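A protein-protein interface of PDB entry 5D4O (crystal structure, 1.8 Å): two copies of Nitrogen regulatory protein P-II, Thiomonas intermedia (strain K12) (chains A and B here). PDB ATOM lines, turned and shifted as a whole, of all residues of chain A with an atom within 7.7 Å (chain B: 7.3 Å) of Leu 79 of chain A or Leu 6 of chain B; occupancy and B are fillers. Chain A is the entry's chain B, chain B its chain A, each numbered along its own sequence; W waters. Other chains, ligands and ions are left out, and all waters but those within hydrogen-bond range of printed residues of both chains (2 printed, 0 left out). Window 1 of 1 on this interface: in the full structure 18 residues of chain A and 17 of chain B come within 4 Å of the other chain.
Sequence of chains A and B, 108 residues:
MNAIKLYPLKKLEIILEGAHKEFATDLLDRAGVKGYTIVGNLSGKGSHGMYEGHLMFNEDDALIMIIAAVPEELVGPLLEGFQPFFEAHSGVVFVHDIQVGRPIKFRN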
ATOM      1  N   LYS A  10      30.698  -8.041   4.758  1.00  0.00           N
ATOM      2  CA  LYS A  10      30.226  -7.794   6.102  1.00  0.00           C
ATOM      3  C   LYS A  10      29.486  -9.045   6.530  1.00  0.00           C
ATOM      4  O   LYS A  10      28.647  -9.546   5.773  1.00  0.00           O
ATOM      5  CB  LYS A  10      29.283  -6.577   6.132  1.00  0.00           C
ATOM      6  CG  LYS A  10      29.963  -5.261   5.774  1.00  0.00           C
ATOM      7  CD  LYS A  10      30.870  -4.714   6.871  1.00  0.00           C
ATOM      8  CE  LYS A  10      31.460  -3.408   6.376  1.00  0.00           C
ATOM      9  NZ  LYS A  10      32.275  -2.740   7.415  1.00  0.00           N
ATOM     10  N   LEU A  12      26.894 -10.526   9.166  1.00  0.00           N
ATOM     11  CA  LEU A  12      25.918 -10.236  10.206  1.00  0.00           C
ATOM     12  C   LEU A  12      25.635 -11.500  11.050  1.00  0.00           C
ATOM     13  O   LEU A  12      25.431 -12.589  10.492  1.00  0.00           O
ATOM     14  CB  LEU A  12      24.589  -9.814   9.547  1.00  0.00           C
ATOM     15  CG  LEU A  12      24.346  -8.363   9.137  1.00  0.00           C
ATOM     16  CD1 LEU A  12      25.608  -7.601   8.761  1.00  0.00           C
ATOM     17  CD2 LEU A  12      23.268  -8.285   8.093  1.00  0.00           C
ATOM     18  N   ILE A  14      22.640 -12.297  13.638  1.00  0.00           N
ATOM     19  CA  ILE A  14      21.338 -11.763  14.058  1.00  0.00           C
ATOM     20  C   ILE A  14      20.756 -12.749  15.045  1.00  0.00           C
ATOM     21  O   ILE A  14      20.402 -13.868  14.654  1.00  0.00           O
ATOM     22  CB  ILE A  14      20.422 -11.588  12.819  1.00  0.00           C
ATOM     23  CG1 ILE A  14      21.077 -10.734  11.721  1.00  0.00           C
ATOM     24  CG2 ILE A  14      19.045 -11.024  13.216  1.00  0.00           C
ATOM     25  CD1 ILE A  14      20.593 -11.190  10.263  1.00  0.00           C
ATOM     26  N   LEU A  27      12.864 -11.101   5.365  1.00  0.00           N
ATOM     27  CA  LEU A  27      13.545  -9.821   5.183  1.00  0.00           C
ATOM     28  C   LEU A  27      14.848 -10.033   4.414  1.00  0.00           C
ATOM     29  O   LEU A  27      15.086  -9.333   3.430  1.00  0.00           O
ATOM     30  CB  LEU A  27      13.822  -9.130   6.539  1.00  0.00           C
ATOM     31  CG  LEU A  27      14.504  -7.758   6.483  1.00  0.00           C
ATOM     32  CD1 LEU A  27      13.758  -6.774   5.592  1.00  0.00           C
ATOM     33  CD2 LEU A  27      14.572  -7.164   7.848  1.00  0.00           C
ATOM     34  N   GLU A  72      28.899  -4.739   1.645  1.00  0.00           N
ATOM     35  CA  GLU A  72      28.729  -3.597   2.562  1.00  0.00           C
ATOM     36  C   GLU A  72      27.495  -2.728   2.238  1.00  0.00           C
ATOM     37  O   GLU A  72      26.840  -2.241   3.162  1.00  0.00           O
ATOM     38  CB  GLU A  72      30.015  -2.741   2.613  1.00  0.00           C
ATOM     39  CG  GLU A  72      29.935  -1.527   3.529  1.00  0.00           C
ATOM     40  CD  GLU A  72      31.218  -0.756   3.777  1.00  0.00           C
ATOM     41  OE1 GLU A  72      32.031  -0.617   2.834  1.00  0.00           O
ATOM     42  OE2 GLU A  72      31.388  -0.254   4.911  1.00  0.00           O
ATOM     43  N   LEU A  74      24.553  -3.624   1.315  1.00  0.00           N
ATOM     44  CA  LEU A  74      23.299  -4.198   1.801  1.00  0.00           C
ATOM     45  C   LEU A  74      23.082  -3.994   3.307  1.00  0.00           C
ATOM     46  O   LEU A  74      21.950  -4.140   3.756  1.00  0.00           O
ATOM     47  CB  LEU A  74      23.139  -5.697   1.426  1.00  0.00           C
ATOM     48  CG  LEU A  74      23.053  -6.102  -0.060  1.00  0.00           C
ATOM     49  CD1 LEU A  74      22.652  -7.564  -0.184  1.00  0.00           C
ATOM     50  CD2 LEU A  74      22.036  -5.232  -0.851  1.00  0.00           C
ATOM     51  N   VAL A  75      24.138  -3.640   4.075  1.00  0.00           N
ATOM     52  CA  VAL A  75      24.046  -3.481   5.547  1.00  0.00           C
ATOM     53  C   VAL A  75      22.986  -2.477   5.985  1.00  0.00           C
ATOM     54  O   VAL A  75      22.073  -2.842   6.718  1.00  0.00           O
ATOM     55  CB  VAL A  75      25.417  -3.264   6.230  1.00  0.00           C
ATOM     56  CG1 VAL A  75      25.260  -3.024   7.739  1.00  0.00           C
ATOM     57  CG2 VAL A  75      26.317  -4.469   5.982  1.00  0.00           C
ATOM     58  N   GLY A  76      23.127  -1.234   5.538  1.00  0.00           N
ATOM     59  CA  GLY A  76      22.198  -0.148   5.862  1.00  0.00           C
ATOM     60  C   GLY A  76      20.748  -0.504   5.578  1.00  0.00           C
ATOM     61  O   GLY A  76      19.952  -0.504   6.519  1.00  0.00           O
ATOM     62  N   PRO A  77      20.384  -0.906   4.327  1.00  0.00           N
ATOM     63  CA  PRO A  77      18.979  -1.281   4.046  1.00  0.00           C
ATOM     64  C   PRO A  77      18.450  -2.445   4.892  1.00  0.00           C
ATOM     65  O   PRO A  77      17.279  -2.410   5.286  1.00  0.00           O
ATOM     66  CB  PRO A  77      18.976  -1.583   2.536  1.00  0.00           C
ATOM     67  CG  PRO A  77      20.159  -0.849   1.995  1.00  0.00           C
ATOM     68  CD  PRO A  77      21.192  -0.938   3.084  1.00  0.00           C
ATOM     69  N   LEU A  78      19.304  -3.441   5.211  1.00  0.00           N
ATOM     70  CA  LEU A  78      18.909  -4.563   6.072  1.00  0.00           C
ATOM     71  C   LEU A  78      18.631  -4.079   7.499  1.00  0.00           C
ATOM     72  O   LEU A  78      17.643  -4.500   8.097  1.00  0.00           O
ATOM     73  CB  LEU A  78      19.974  -5.679   6.113  1.00  0.00           C
ATOM     74  CG  LEU A  78      19.922  -6.718   4.981  1.00  0.00           C
ATOM     75  CD1 LEU A  78      21.214  -7.565   4.958  1.00  0.00           C
ATOM     76  CD2 LEU A  78      18.688  -7.637   5.126  1.00  0.00           C
ATOM     77  N   LEU A  79      19.512  -3.229   8.055  1.00  0.00           N
ATOM     78  CA  LEU A  79      19.316  -2.714   9.421  1.00  0.00           C
ATOM     79  C   LEU A  79      18.065  -1.855   9.505  1.00  0.00           C
ATOM     80  O   LEU A  79      17.359  -1.887  10.514  1.00  0.00           O
ATOM     81  CB  LEU A  79      20.529  -1.940   9.932  1.00  0.00           C
ATOM     82  CG  LEU A  79      21.848  -2.731  10.078  1.00  0.00           C
ATOM     83  CD1 LEU A  79      22.928  -1.844  10.651  1.00  0.00           C
ATOM     84  CD2 LEU A  79      21.672  -3.962  10.959  1.00  0.00           C
ATOM     85  N   GLU A  80      17.790  -1.083   8.439  1.00  0.00           N
ATOM     86  CA  GLU A  80      16.577  -0.269   8.350  1.00  0.00           C
ATOM     87  C   GLU A  80      15.354  -1.200   8.382  1.00  0.00           C
ATOM     88  O   GLU A  80      14.366  -0.900   9.055  1.00  0.00           O
ATOM     89  CB  GLU A  80      16.572   0.537   7.041  1.00  0.00           C
ATOM     90  CG  GLU A  80      17.477   1.755   7.078  1.00  0.00           C
ATOM     91  CD  GLU A  80      17.400   2.631   5.840  1.00  0.00           C
ATOM     92  OE1 GLU A  80      16.292   2.775   5.275  1.00  0.00           O
ATOM     93  OE2 GLU A  80      18.451   3.183   5.445  1.00  0.00           O
ATOM     94  N   GLY A  81      15.430  -2.309   7.644  1.00  0.00           N
ATOM     95  CA  GLY A  81      14.359  -3.301   7.597  1.00  0.00           C
ATOM     96  C   GLY A  81      14.162  -3.959   8.959  1.00  0.00           C
ATOM     97  O   GLY A  81      13.027  -4.216   9.355  1.00  0.00           O
ATOM     98  N   PHE A  82      15.268  -4.231   9.695  1.00  0.00           N
ATOM     99  CA  PHE A  82      15.195  -4.870  11.019  1.00  0.00           C
ATOM    100  C   PHE A  82      14.841  -3.897  12.143  1.00  0.00           C
ATOM    101  O   PHE A  82      14.419  -4.338  13.210  1.00  0.00           O
ATOM    102  CB  PHE A  82      16.507  -5.582  11.379  1.00  0.00           C
ATOM    103  CG  PHE A  82      16.618  -6.995  10.843  1.00  0.00           C
ATOM    104  CD1 PHE A  82      15.893  -8.037  11.423  1.00  0.00           C
ATOM    105  CD2 PHE A  82      17.491  -7.295   9.801  1.00  0.00           C
ATOM    106  CE1 PHE A  82      16.014  -9.353  10.944  1.00  0.00           C
ATOM    107  CE2 PHE A  82      17.598  -8.606   9.305  1.00  0.00           C
ATOM    108  CZ  PHE A  82      16.866  -9.626   9.886  1.00  0.00           C
ATOM    109  N   GLN A  83      15.068  -2.588  11.927  1.00  0.00           N
ATOM    110  CA  GLN A  83      14.838  -1.554  12.955  1.00  0.00           C
ATOM    111  C   GLN A  83      13.451  -1.641  13.658  1.00  0.00           C
ATOM    112  O   GLN A  83      13.452  -1.741  14.893  1.00  0.00           O
ATOM    113  CB  GLN A  83      15.081  -0.141  12.382  1.00  0.00           C
ATOM    114  CG  GLN A  83      14.873   0.951  13.424  1.00  0.00           C
ATOM    115  CD  GLN A  83      15.050   2.331  12.874  1.00  0.00           C
ATOM    116  OE1 GLN A  83      14.993   2.561  11.667  1.00  0.00           O
ATOM    117  NE2 GLN A  83      15.191   3.290  13.764  1.00  0.00           N
ATOM    118  N   PRO A  84      12.289  -1.606  12.937  1.00  0.00           N
ATOM    119  CA  PRO A  84      10.988  -1.683  13.639  1.00  0.00           C
ATOM    120  C   PRO A  84      10.855  -2.924  14.502  1.00  0.00           C
ATOM    121  O   PRO A  84      10.301  -2.842  15.589  1.00  0.00           O
ATOM    122  CB  PRO A  84       9.964  -1.706  12.505  1.00  0.00           C
ATOM    123  CG  PRO A  84      10.663  -1.130  11.335  1.00  0.00           C
ATOM    124  CD  PRO A  84      12.091  -1.482  11.473  1.00  0.00           C
ATOM    125  N   PHE A  85      11.384  -4.064  14.034  1.00  0.00           N
ATOM    126  CA  PHE A  85      11.344  -5.314  14.788  1.00  0.00           C
ATOM    127  C   PHE A  85      12.160  -5.213  16.086  1.00  0.00           C
ATOM    128  O   PHE A  85      11.638  -5.518  17.152  1.00  0.00           O
ATOM    129  CB  PHE A  85      11.829  -6.497  13.921  1.00  0.00           C
ATOM    130  CG  PHE A  85      11.967  -7.777  14.713  1.00  0.00           C
ATOM    131  CD1 PHE A  85      10.856  -8.567  14.987  1.00  0.00           C
ATOM    132  CD2 PHE A  85      13.204  -8.177  15.210  1.00  0.00           C
ATOM    133  CE1 PHE A  85      10.975  -9.722  15.761  1.00  0.00           C
ATOM    134  CE2 PHE A  85      13.322  -9.334  15.989  1.00  0.00           C
ATOM    135  CZ  PHE A  85      12.208 -10.092  16.267  1.00  0.00           C
ATOM    136  N   PHE A  86      13.436  -4.801  15.988  1.00  0.00           N
ATOM    137  CA  PHE A  86      14.314  -4.690  17.143  1.00  0.00           C
ATOM    138  C   PHE A  86      13.937  -3.625  18.150  1.00  0.00           C
ATOM    139  O   PHE A  86      14.356  -3.727  19.309  1.00  0.00           O
ATOM    140  CB  PHE A  86      15.802  -4.649  16.765  1.00  0.00           C
ATOM    141  CG  PHE A  86      16.346  -5.991  16.322  1.00  0.00           C
ATOM    142  CD1 PHE A  86      16.195  -7.129  17.126  1.00  0.00           C
ATOM    143  CD2 PHE A  86      17.021  -6.119  15.115  1.00  0.00           C
ATOM    144  CE1 PHE A  86      16.712  -8.371  16.725  1.00  0.00           C
ATOM    145  CE2 PHE A  86      17.537  -7.364  14.709  1.00  0.00           C
ATOM    146  CZ  PHE A  86      17.371  -8.481  15.513  1.00  0.00           C
ATOM    147  N   VAL A  93      22.044  -7.484  16.765  1.00  0.00           N
ATOM    148  CA  VAL A  93      22.727  -7.690  15.477  1.00  0.00           C
ATOM    149  C   VAL A  93      24.179  -7.271  15.676  1.00  0.00           C
ATOM    150  O   VAL A  93      24.427  -6.158  16.152  1.00  0.00           O
ATOM    151  CB  VAL A  93      22.140  -6.922  14.266  1.00  0.00           C
ATOM    152  CG1 VAL A  93      22.890  -7.279  12.983  1.00  0.00           C
ATOM    153  CG2 VAL A  93      20.661  -7.203  14.098  1.00  0.00           C
ATOM    154  N   PHE A  94      25.122  -8.144  15.308  1.00  0.00           N
ATOM    155  CA  PHE A  94      26.568  -7.852  15.364  1.00  0.00           C
ATOM    156  C   PHE A  94      27.077  -7.802  13.933  1.00  0.00           C
ATOM    157  O   PHE A  94      26.821  -8.727  13.168  1.00  0.00           O
ATOM    158  CB  PHE A  94      27.324  -8.955  16.106  1.00  0.00           C
ATOM    159  CG  PHE A  94      26.832  -9.248  17.494  1.00  0.00           C
ATOM    160  CD1 PHE A  94      26.333  -8.229  18.303  1.00  0.00           C
ATOM    161  CD2 PHE A  94      26.914 -10.537  18.014  1.00  0.00           C
ATOM    162  CE1 PHE A  94      25.905  -8.504  19.605  1.00  0.00           C
ATOM    163  CE2 PHE A  94      26.494 -10.803  19.314  1.00  0.00           C
ATOM    164  CZ  PHE A  94      25.993  -9.797  20.094  1.00  0.00           C
ATOM    165  N   VAL A  95      27.752  -6.713  13.551  1.00  0.00           N
ATOM    166  CA  VAL A  95      28.277  -6.600  12.187  1.00  0.00           C
ATOM    167  C   VAL A  95      29.806  -6.855  12.245  1.00  0.00           C
ATOM    168  O   VAL A  95      30.503  -6.169  12.989  1.00  0.00           O
ATOM    169  CB  VAL A  95      27.947  -5.193  11.569  1.00  0.00           C
ATOM    170  CG1 VAL A  95      28.478  -5.087  10.128  1.00  0.00           C
ATOM    171  CG2 VAL A  95      26.439  -4.910  11.605  1.00  0.00           C
ATOM    172  N   ALA B   3      21.424   6.240   7.682  1.00  0.00           N
ATOM    173  CA  ALA B   3      20.271   6.363   8.577  1.00  0.00           C
ATOM    174  C   ALA B   3      20.525   5.655   9.912  1.00  0.00           C
ATOM    175  O   ALA B   3      20.334   6.271  10.961  1.00  0.00           O
ATOM    176  CB  ALA B   3      19.014   5.816   7.913  1.00  0.00           C
ATOM    177  N   ILE B   4      20.962   4.380   9.881  1.00  0.00           N
ATOM    178  CA  ILE B   4      21.267   3.653  11.113  1.00  0.00           C
ATOM    179  C   ILE B   4      22.757   3.742  11.411  1.00  0.00           C
ATOM    180  O   ILE B   4      23.579   3.141  10.703  1.00  0.00           O
ATOM    181  CB  ILE B   4      20.666   2.217  11.171  1.00  0.00           C
ATOM    182  CG1 ILE B   4      19.111   2.318  11.180  1.00  0.00           C
ATOM    183  CG2 ILE B   4      21.199   1.431  12.415  1.00  0.00           C
ATOM    184  CD1 ILE B   4      18.372   1.122  11.404  1.00  0.00           C
ATOM    185  N   LYS B   5      23.100   4.518  12.456  1.00  0.00           N
ATOM    186  CA  LYS B   5      24.488   4.707  12.875  1.00  0.00           C
ATOM    187  C   LYS B   5      25.050   3.428  13.475  1.00  0.00           C
ATOM    188  O   LYS B   5      24.341   2.705  14.183  1.00  0.00           O
ATOM    189  CB  LYS B   5      24.628   5.863  13.889  1.00  0.00           C
ATOM    190  CG  LYS B   5      24.119   7.224  13.374  1.00  0.00           C
ATOM    191  CD  LYS B   5      24.840   7.708  12.116  1.00  0.00           C
ATOM    192  CE  LYS B   5      24.157   8.901  11.487  1.00  0.00           C
ATOM    193  NZ  LYS B   5      24.780   9.267  10.188  1.00  0.00           N
ATOM    194  N   LEU B   6      26.316   3.151  13.183  1.00  0.00           N
ATOM    195  CA  LEU B   6      27.000   1.980  13.724  1.00  0.00           C
ATOM    196  C   LEU B   6      28.134   2.428  14.612  1.00  0.00           C
ATOM    197  O   LEU B   6      28.755   3.467  14.351  1.00  0.00           O
ATOM    198  CB  LEU B   6      27.490   1.049  12.610  1.00  0.00           C
ATOM    199  CG  LEU B   6      26.402   0.219  11.916  1.00  0.00           C
ATOM    200  CD1 LEU B   6      26.990  -0.573  10.758  1.00  0.00           C
ATOM    201  CD2 LEU B   6      25.727  -0.735  12.890  1.00  0.00           C
ATOM    202  N   TYR B   7      28.375   1.676  15.690  1.00  0.00           N
ATOM    203  CA  TYR B   7      29.367   2.017  16.700  1.00  0.00           C
ATOM    204  C   TYR B   7      30.275   0.813  16.973  1.00  0.00           C
ATOM    205  O   TYR B   7      29.774  -0.320  16.959  1.00  0.00           O
ATOM    206  CB  TYR B   7      28.651   2.418  18.004  1.00  0.00           C
ATOM    207  CG  TYR B   7      27.669   3.566  17.857  1.00  0.00           C
ATOM    208  CD1 TYR B   7      26.355   3.337  17.455  1.00  0.00           C
ATOM    209  CD2 TYR B   7      28.028   4.864  18.204  1.00  0.00           C
ATOM    210  CE1 TYR B   7      25.434   4.385  17.349  1.00  0.00           C
ATOM    211  CE2 TYR B   7      27.115   5.921  18.109  1.00  0.00           C
ATOM    212  CZ  TYR B   7      25.820   5.675  17.674  1.00  0.00           C
ATOM    213  OH  TYR B   7      24.916   6.702  17.567  1.00  0.00           O
ATOM    214  N   PRO B   8      31.570   1.039  17.307  1.00  0.00           N
ATOM    215  CA  PRO B   8      32.468  -0.096  17.593  1.00  0.00           C
ATOM    216  C   PRO B   8      32.218  -0.766  18.935  1.00  0.00           C
ATOM    217  O   PRO B   8      31.927  -0.109  19.930  1.00  0.00           O
ATOM    218  CB  PRO B   8      33.863   0.540  17.576  1.00  0.00           C
ATOM    219  CG  PRO B   8      33.623   1.972  17.975  1.00  0.00           C
ATOM    220  CD  PRO B   8      32.300   2.333  17.361  1.00  0.00           C
ATOM    221  N   GLN B  99      30.582  -4.118  15.006  1.00  0.00           N
ATOM    222  CA  GLN B  99      29.825  -2.852  14.970  1.00  0.00           C
ATOM    223  C   GLN B  99      28.407  -3.181  15.427  1.00  0.00           C
ATOM    224  O   GLN B  99      27.882  -4.254  15.075  1.00  0.00           O
ATOM    225  CB  GLN B  99      29.745  -2.247  13.551  1.00  0.00           C
ATOM    226  CG  GLN B  99      30.972  -1.451  13.100  1.00  0.00           C
ATOM    227  CD  GLN B  99      30.802  -0.906  11.694  1.00  0.00           C
ATOM    228  OE1 GLN B  99      30.663   0.308  11.468  1.00  0.00           O
ATOM    229  NE2 GLN B  99      30.806  -1.792  10.705  1.00  0.00           N
ATOM    230  N   VAL B 100      27.796  -2.311  16.223  1.00  0.00           N
ATOM    231  CA  VAL B 100      26.423  -2.483  16.706  1.00  0.00           C
ATOM    232  C   VAL B 100      25.683  -1.183  16.498  1.00  0.00           C
ATOM    233  O   VAL B 100      26.312  -0.115  16.375  1.00  0.00           O
ATOM    234  CB  VAL B 100      26.325  -2.941  18.208  1.00  0.00           C
ATOM    235  CG1 VAL B 100      27.038  -4.287  18.434  1.00  0.00           C
ATOM    236  CG2 VAL B 100      26.855  -1.858  19.166  1.00  0.00           C
ATOM    237  N   GLY B 101      24.353  -1.259  16.499  1.00  0.00           N
ATOM    238  CA  GLY B 101      23.529  -0.069  16.340  1.00  0.00           C
ATOM    239  C   GLY B 101      23.171   0.632  17.631  1.00  0.00           C
ATOM    240  O   GLY B 101      22.873   1.824  17.603  1.00  0.00           O
ATOM    241  N   ARG B 102      23.196  -0.100  18.777  1.00  0.00           N
ATOM    242  CA  ARG B 102      22.715   0.426  20.057  1.00  0.00           C
ATOM    243  C   ARG B 102      23.697   0.227  21.219  1.00  0.00           C
ATOM    244  O   ARG B 102      23.540  -0.712  22.008  1.00  0.00           O
ATOM    245  CB  ARG B 102      21.333  -0.191  20.380  1.00  0.00           C
ATOM    246  CG  ARG B 102      20.270   0.110  19.312  1.00  0.00           C
ATOM    247  CD  ARG B 102      19.056  -0.789  19.461  1.00  0.00           C
ATOM    248  NE  ARG B 102      19.377  -2.196  19.196  1.00  0.00           N
ATOM    249  CZ  ARG B 102      18.506  -3.187  19.323  1.00  0.00           C
ATOM    250  NH1 ARG B 102      17.246  -2.935  19.683  1.00  0.00           N
ATOM    251  NH2 ARG B 102      18.882  -4.437  19.096  1.00  0.00           N
ATOM    252  N   PRO B 103      24.707   1.126  21.349  1.00  0.00           N
ATOM    253  CA  PRO B 103      25.699   0.987  22.432  1.00  0.00           C
ATOM    254  C   PRO B 103      25.107   0.898  23.831  1.00  0.00           C
ATOM    255  O   PRO B 103      25.648   0.173  24.645  1.00  0.00           O
ATOM    256  CB  PRO B 103      26.572   2.244  22.296  1.00  0.00           C
ATOM    257  CG  PRO B 103      26.349   2.739  20.964  1.00  0.00           C
ATOM    258  CD  PRO B 103      25.010   2.284  20.488  1.00  0.00           C
HETATM  259  O   HOH W   1      31.692  -4.272  10.972  1.00  0.00           O
HETATM  260  O   HOH W   2      16.257  -5.800  20.473  1.00  0.00           O
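The backbone NH of Gln 99 of chain B is in hydrogen-bond range of the backbone carbonyl oxygen of Val 95 of chain A (2.9 Å). The guanidinium group (NH1) of Arg 102 of chain B lies within hydrogen-bond range of the backbone carbonyl oxygen (O) of Phe 86 of chain A, 3.0 Å away.
N of Tyr 7 of chain B sits at hydrogen-bond distance from O of Val 100 of chain B (2.8 Å). NZ of Lys 10 of chain A is in salt-bridge range of OE2 of Glu 72 of chain A.
Among the printed residues, pairs that only touch across the chains: Lys 10 of chain A with Gln 99 of chain B, Leu 79 of chain A with Ile 4 of chain B, Leu 79 of chain A with Leu 6 of chain B, Glu 80 of chain A with Ala 3 of chain B, Glu 80 of chain A with Ile 4 of chain B, Gln 83 of chain A with Ile 4 of chain B, Val 93 of chain A with Val 100 of chain B and Phe 94 of chain A with Gln 99 of chain B.
Of chain B, only Ile 4 and Leu 6 come within 4 Å of Leu 79 of chain A. Printed residues of chain B within 4 Å of Val 93 of chain A: Val 100. Of the printed residues of chain B, Phe 94 of chain A touches Gln 99. Printed residues of chain B within 4 Å of Gln 83 of chain A: Ile 4 (3.7 Å). Printed residues of chain A within 4 Å of Val 100 of chain B: Val 93. Printed residues of chain A within 4 Å of Ala 3 of chain B: Glu 80. The nearest residue of chain A that does not touch Leu 6 of chain B is Val 75 of chain A (4.3 Å).
No position is printed for both chains. Of the 10 pairs that touch across the chains among the printed residues, none has its exchanged pair printed and touching as well.
Water W1 lies within hydrogen-bond range of NE2 of Gln 99 of chain B and O of Val 95 of chain A. Water W2 lies within hydrogen-bond range of O of Phe 86 of chain A (3.0 Å) and NH1 of Arg 102 of chain B (3.1 Å).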
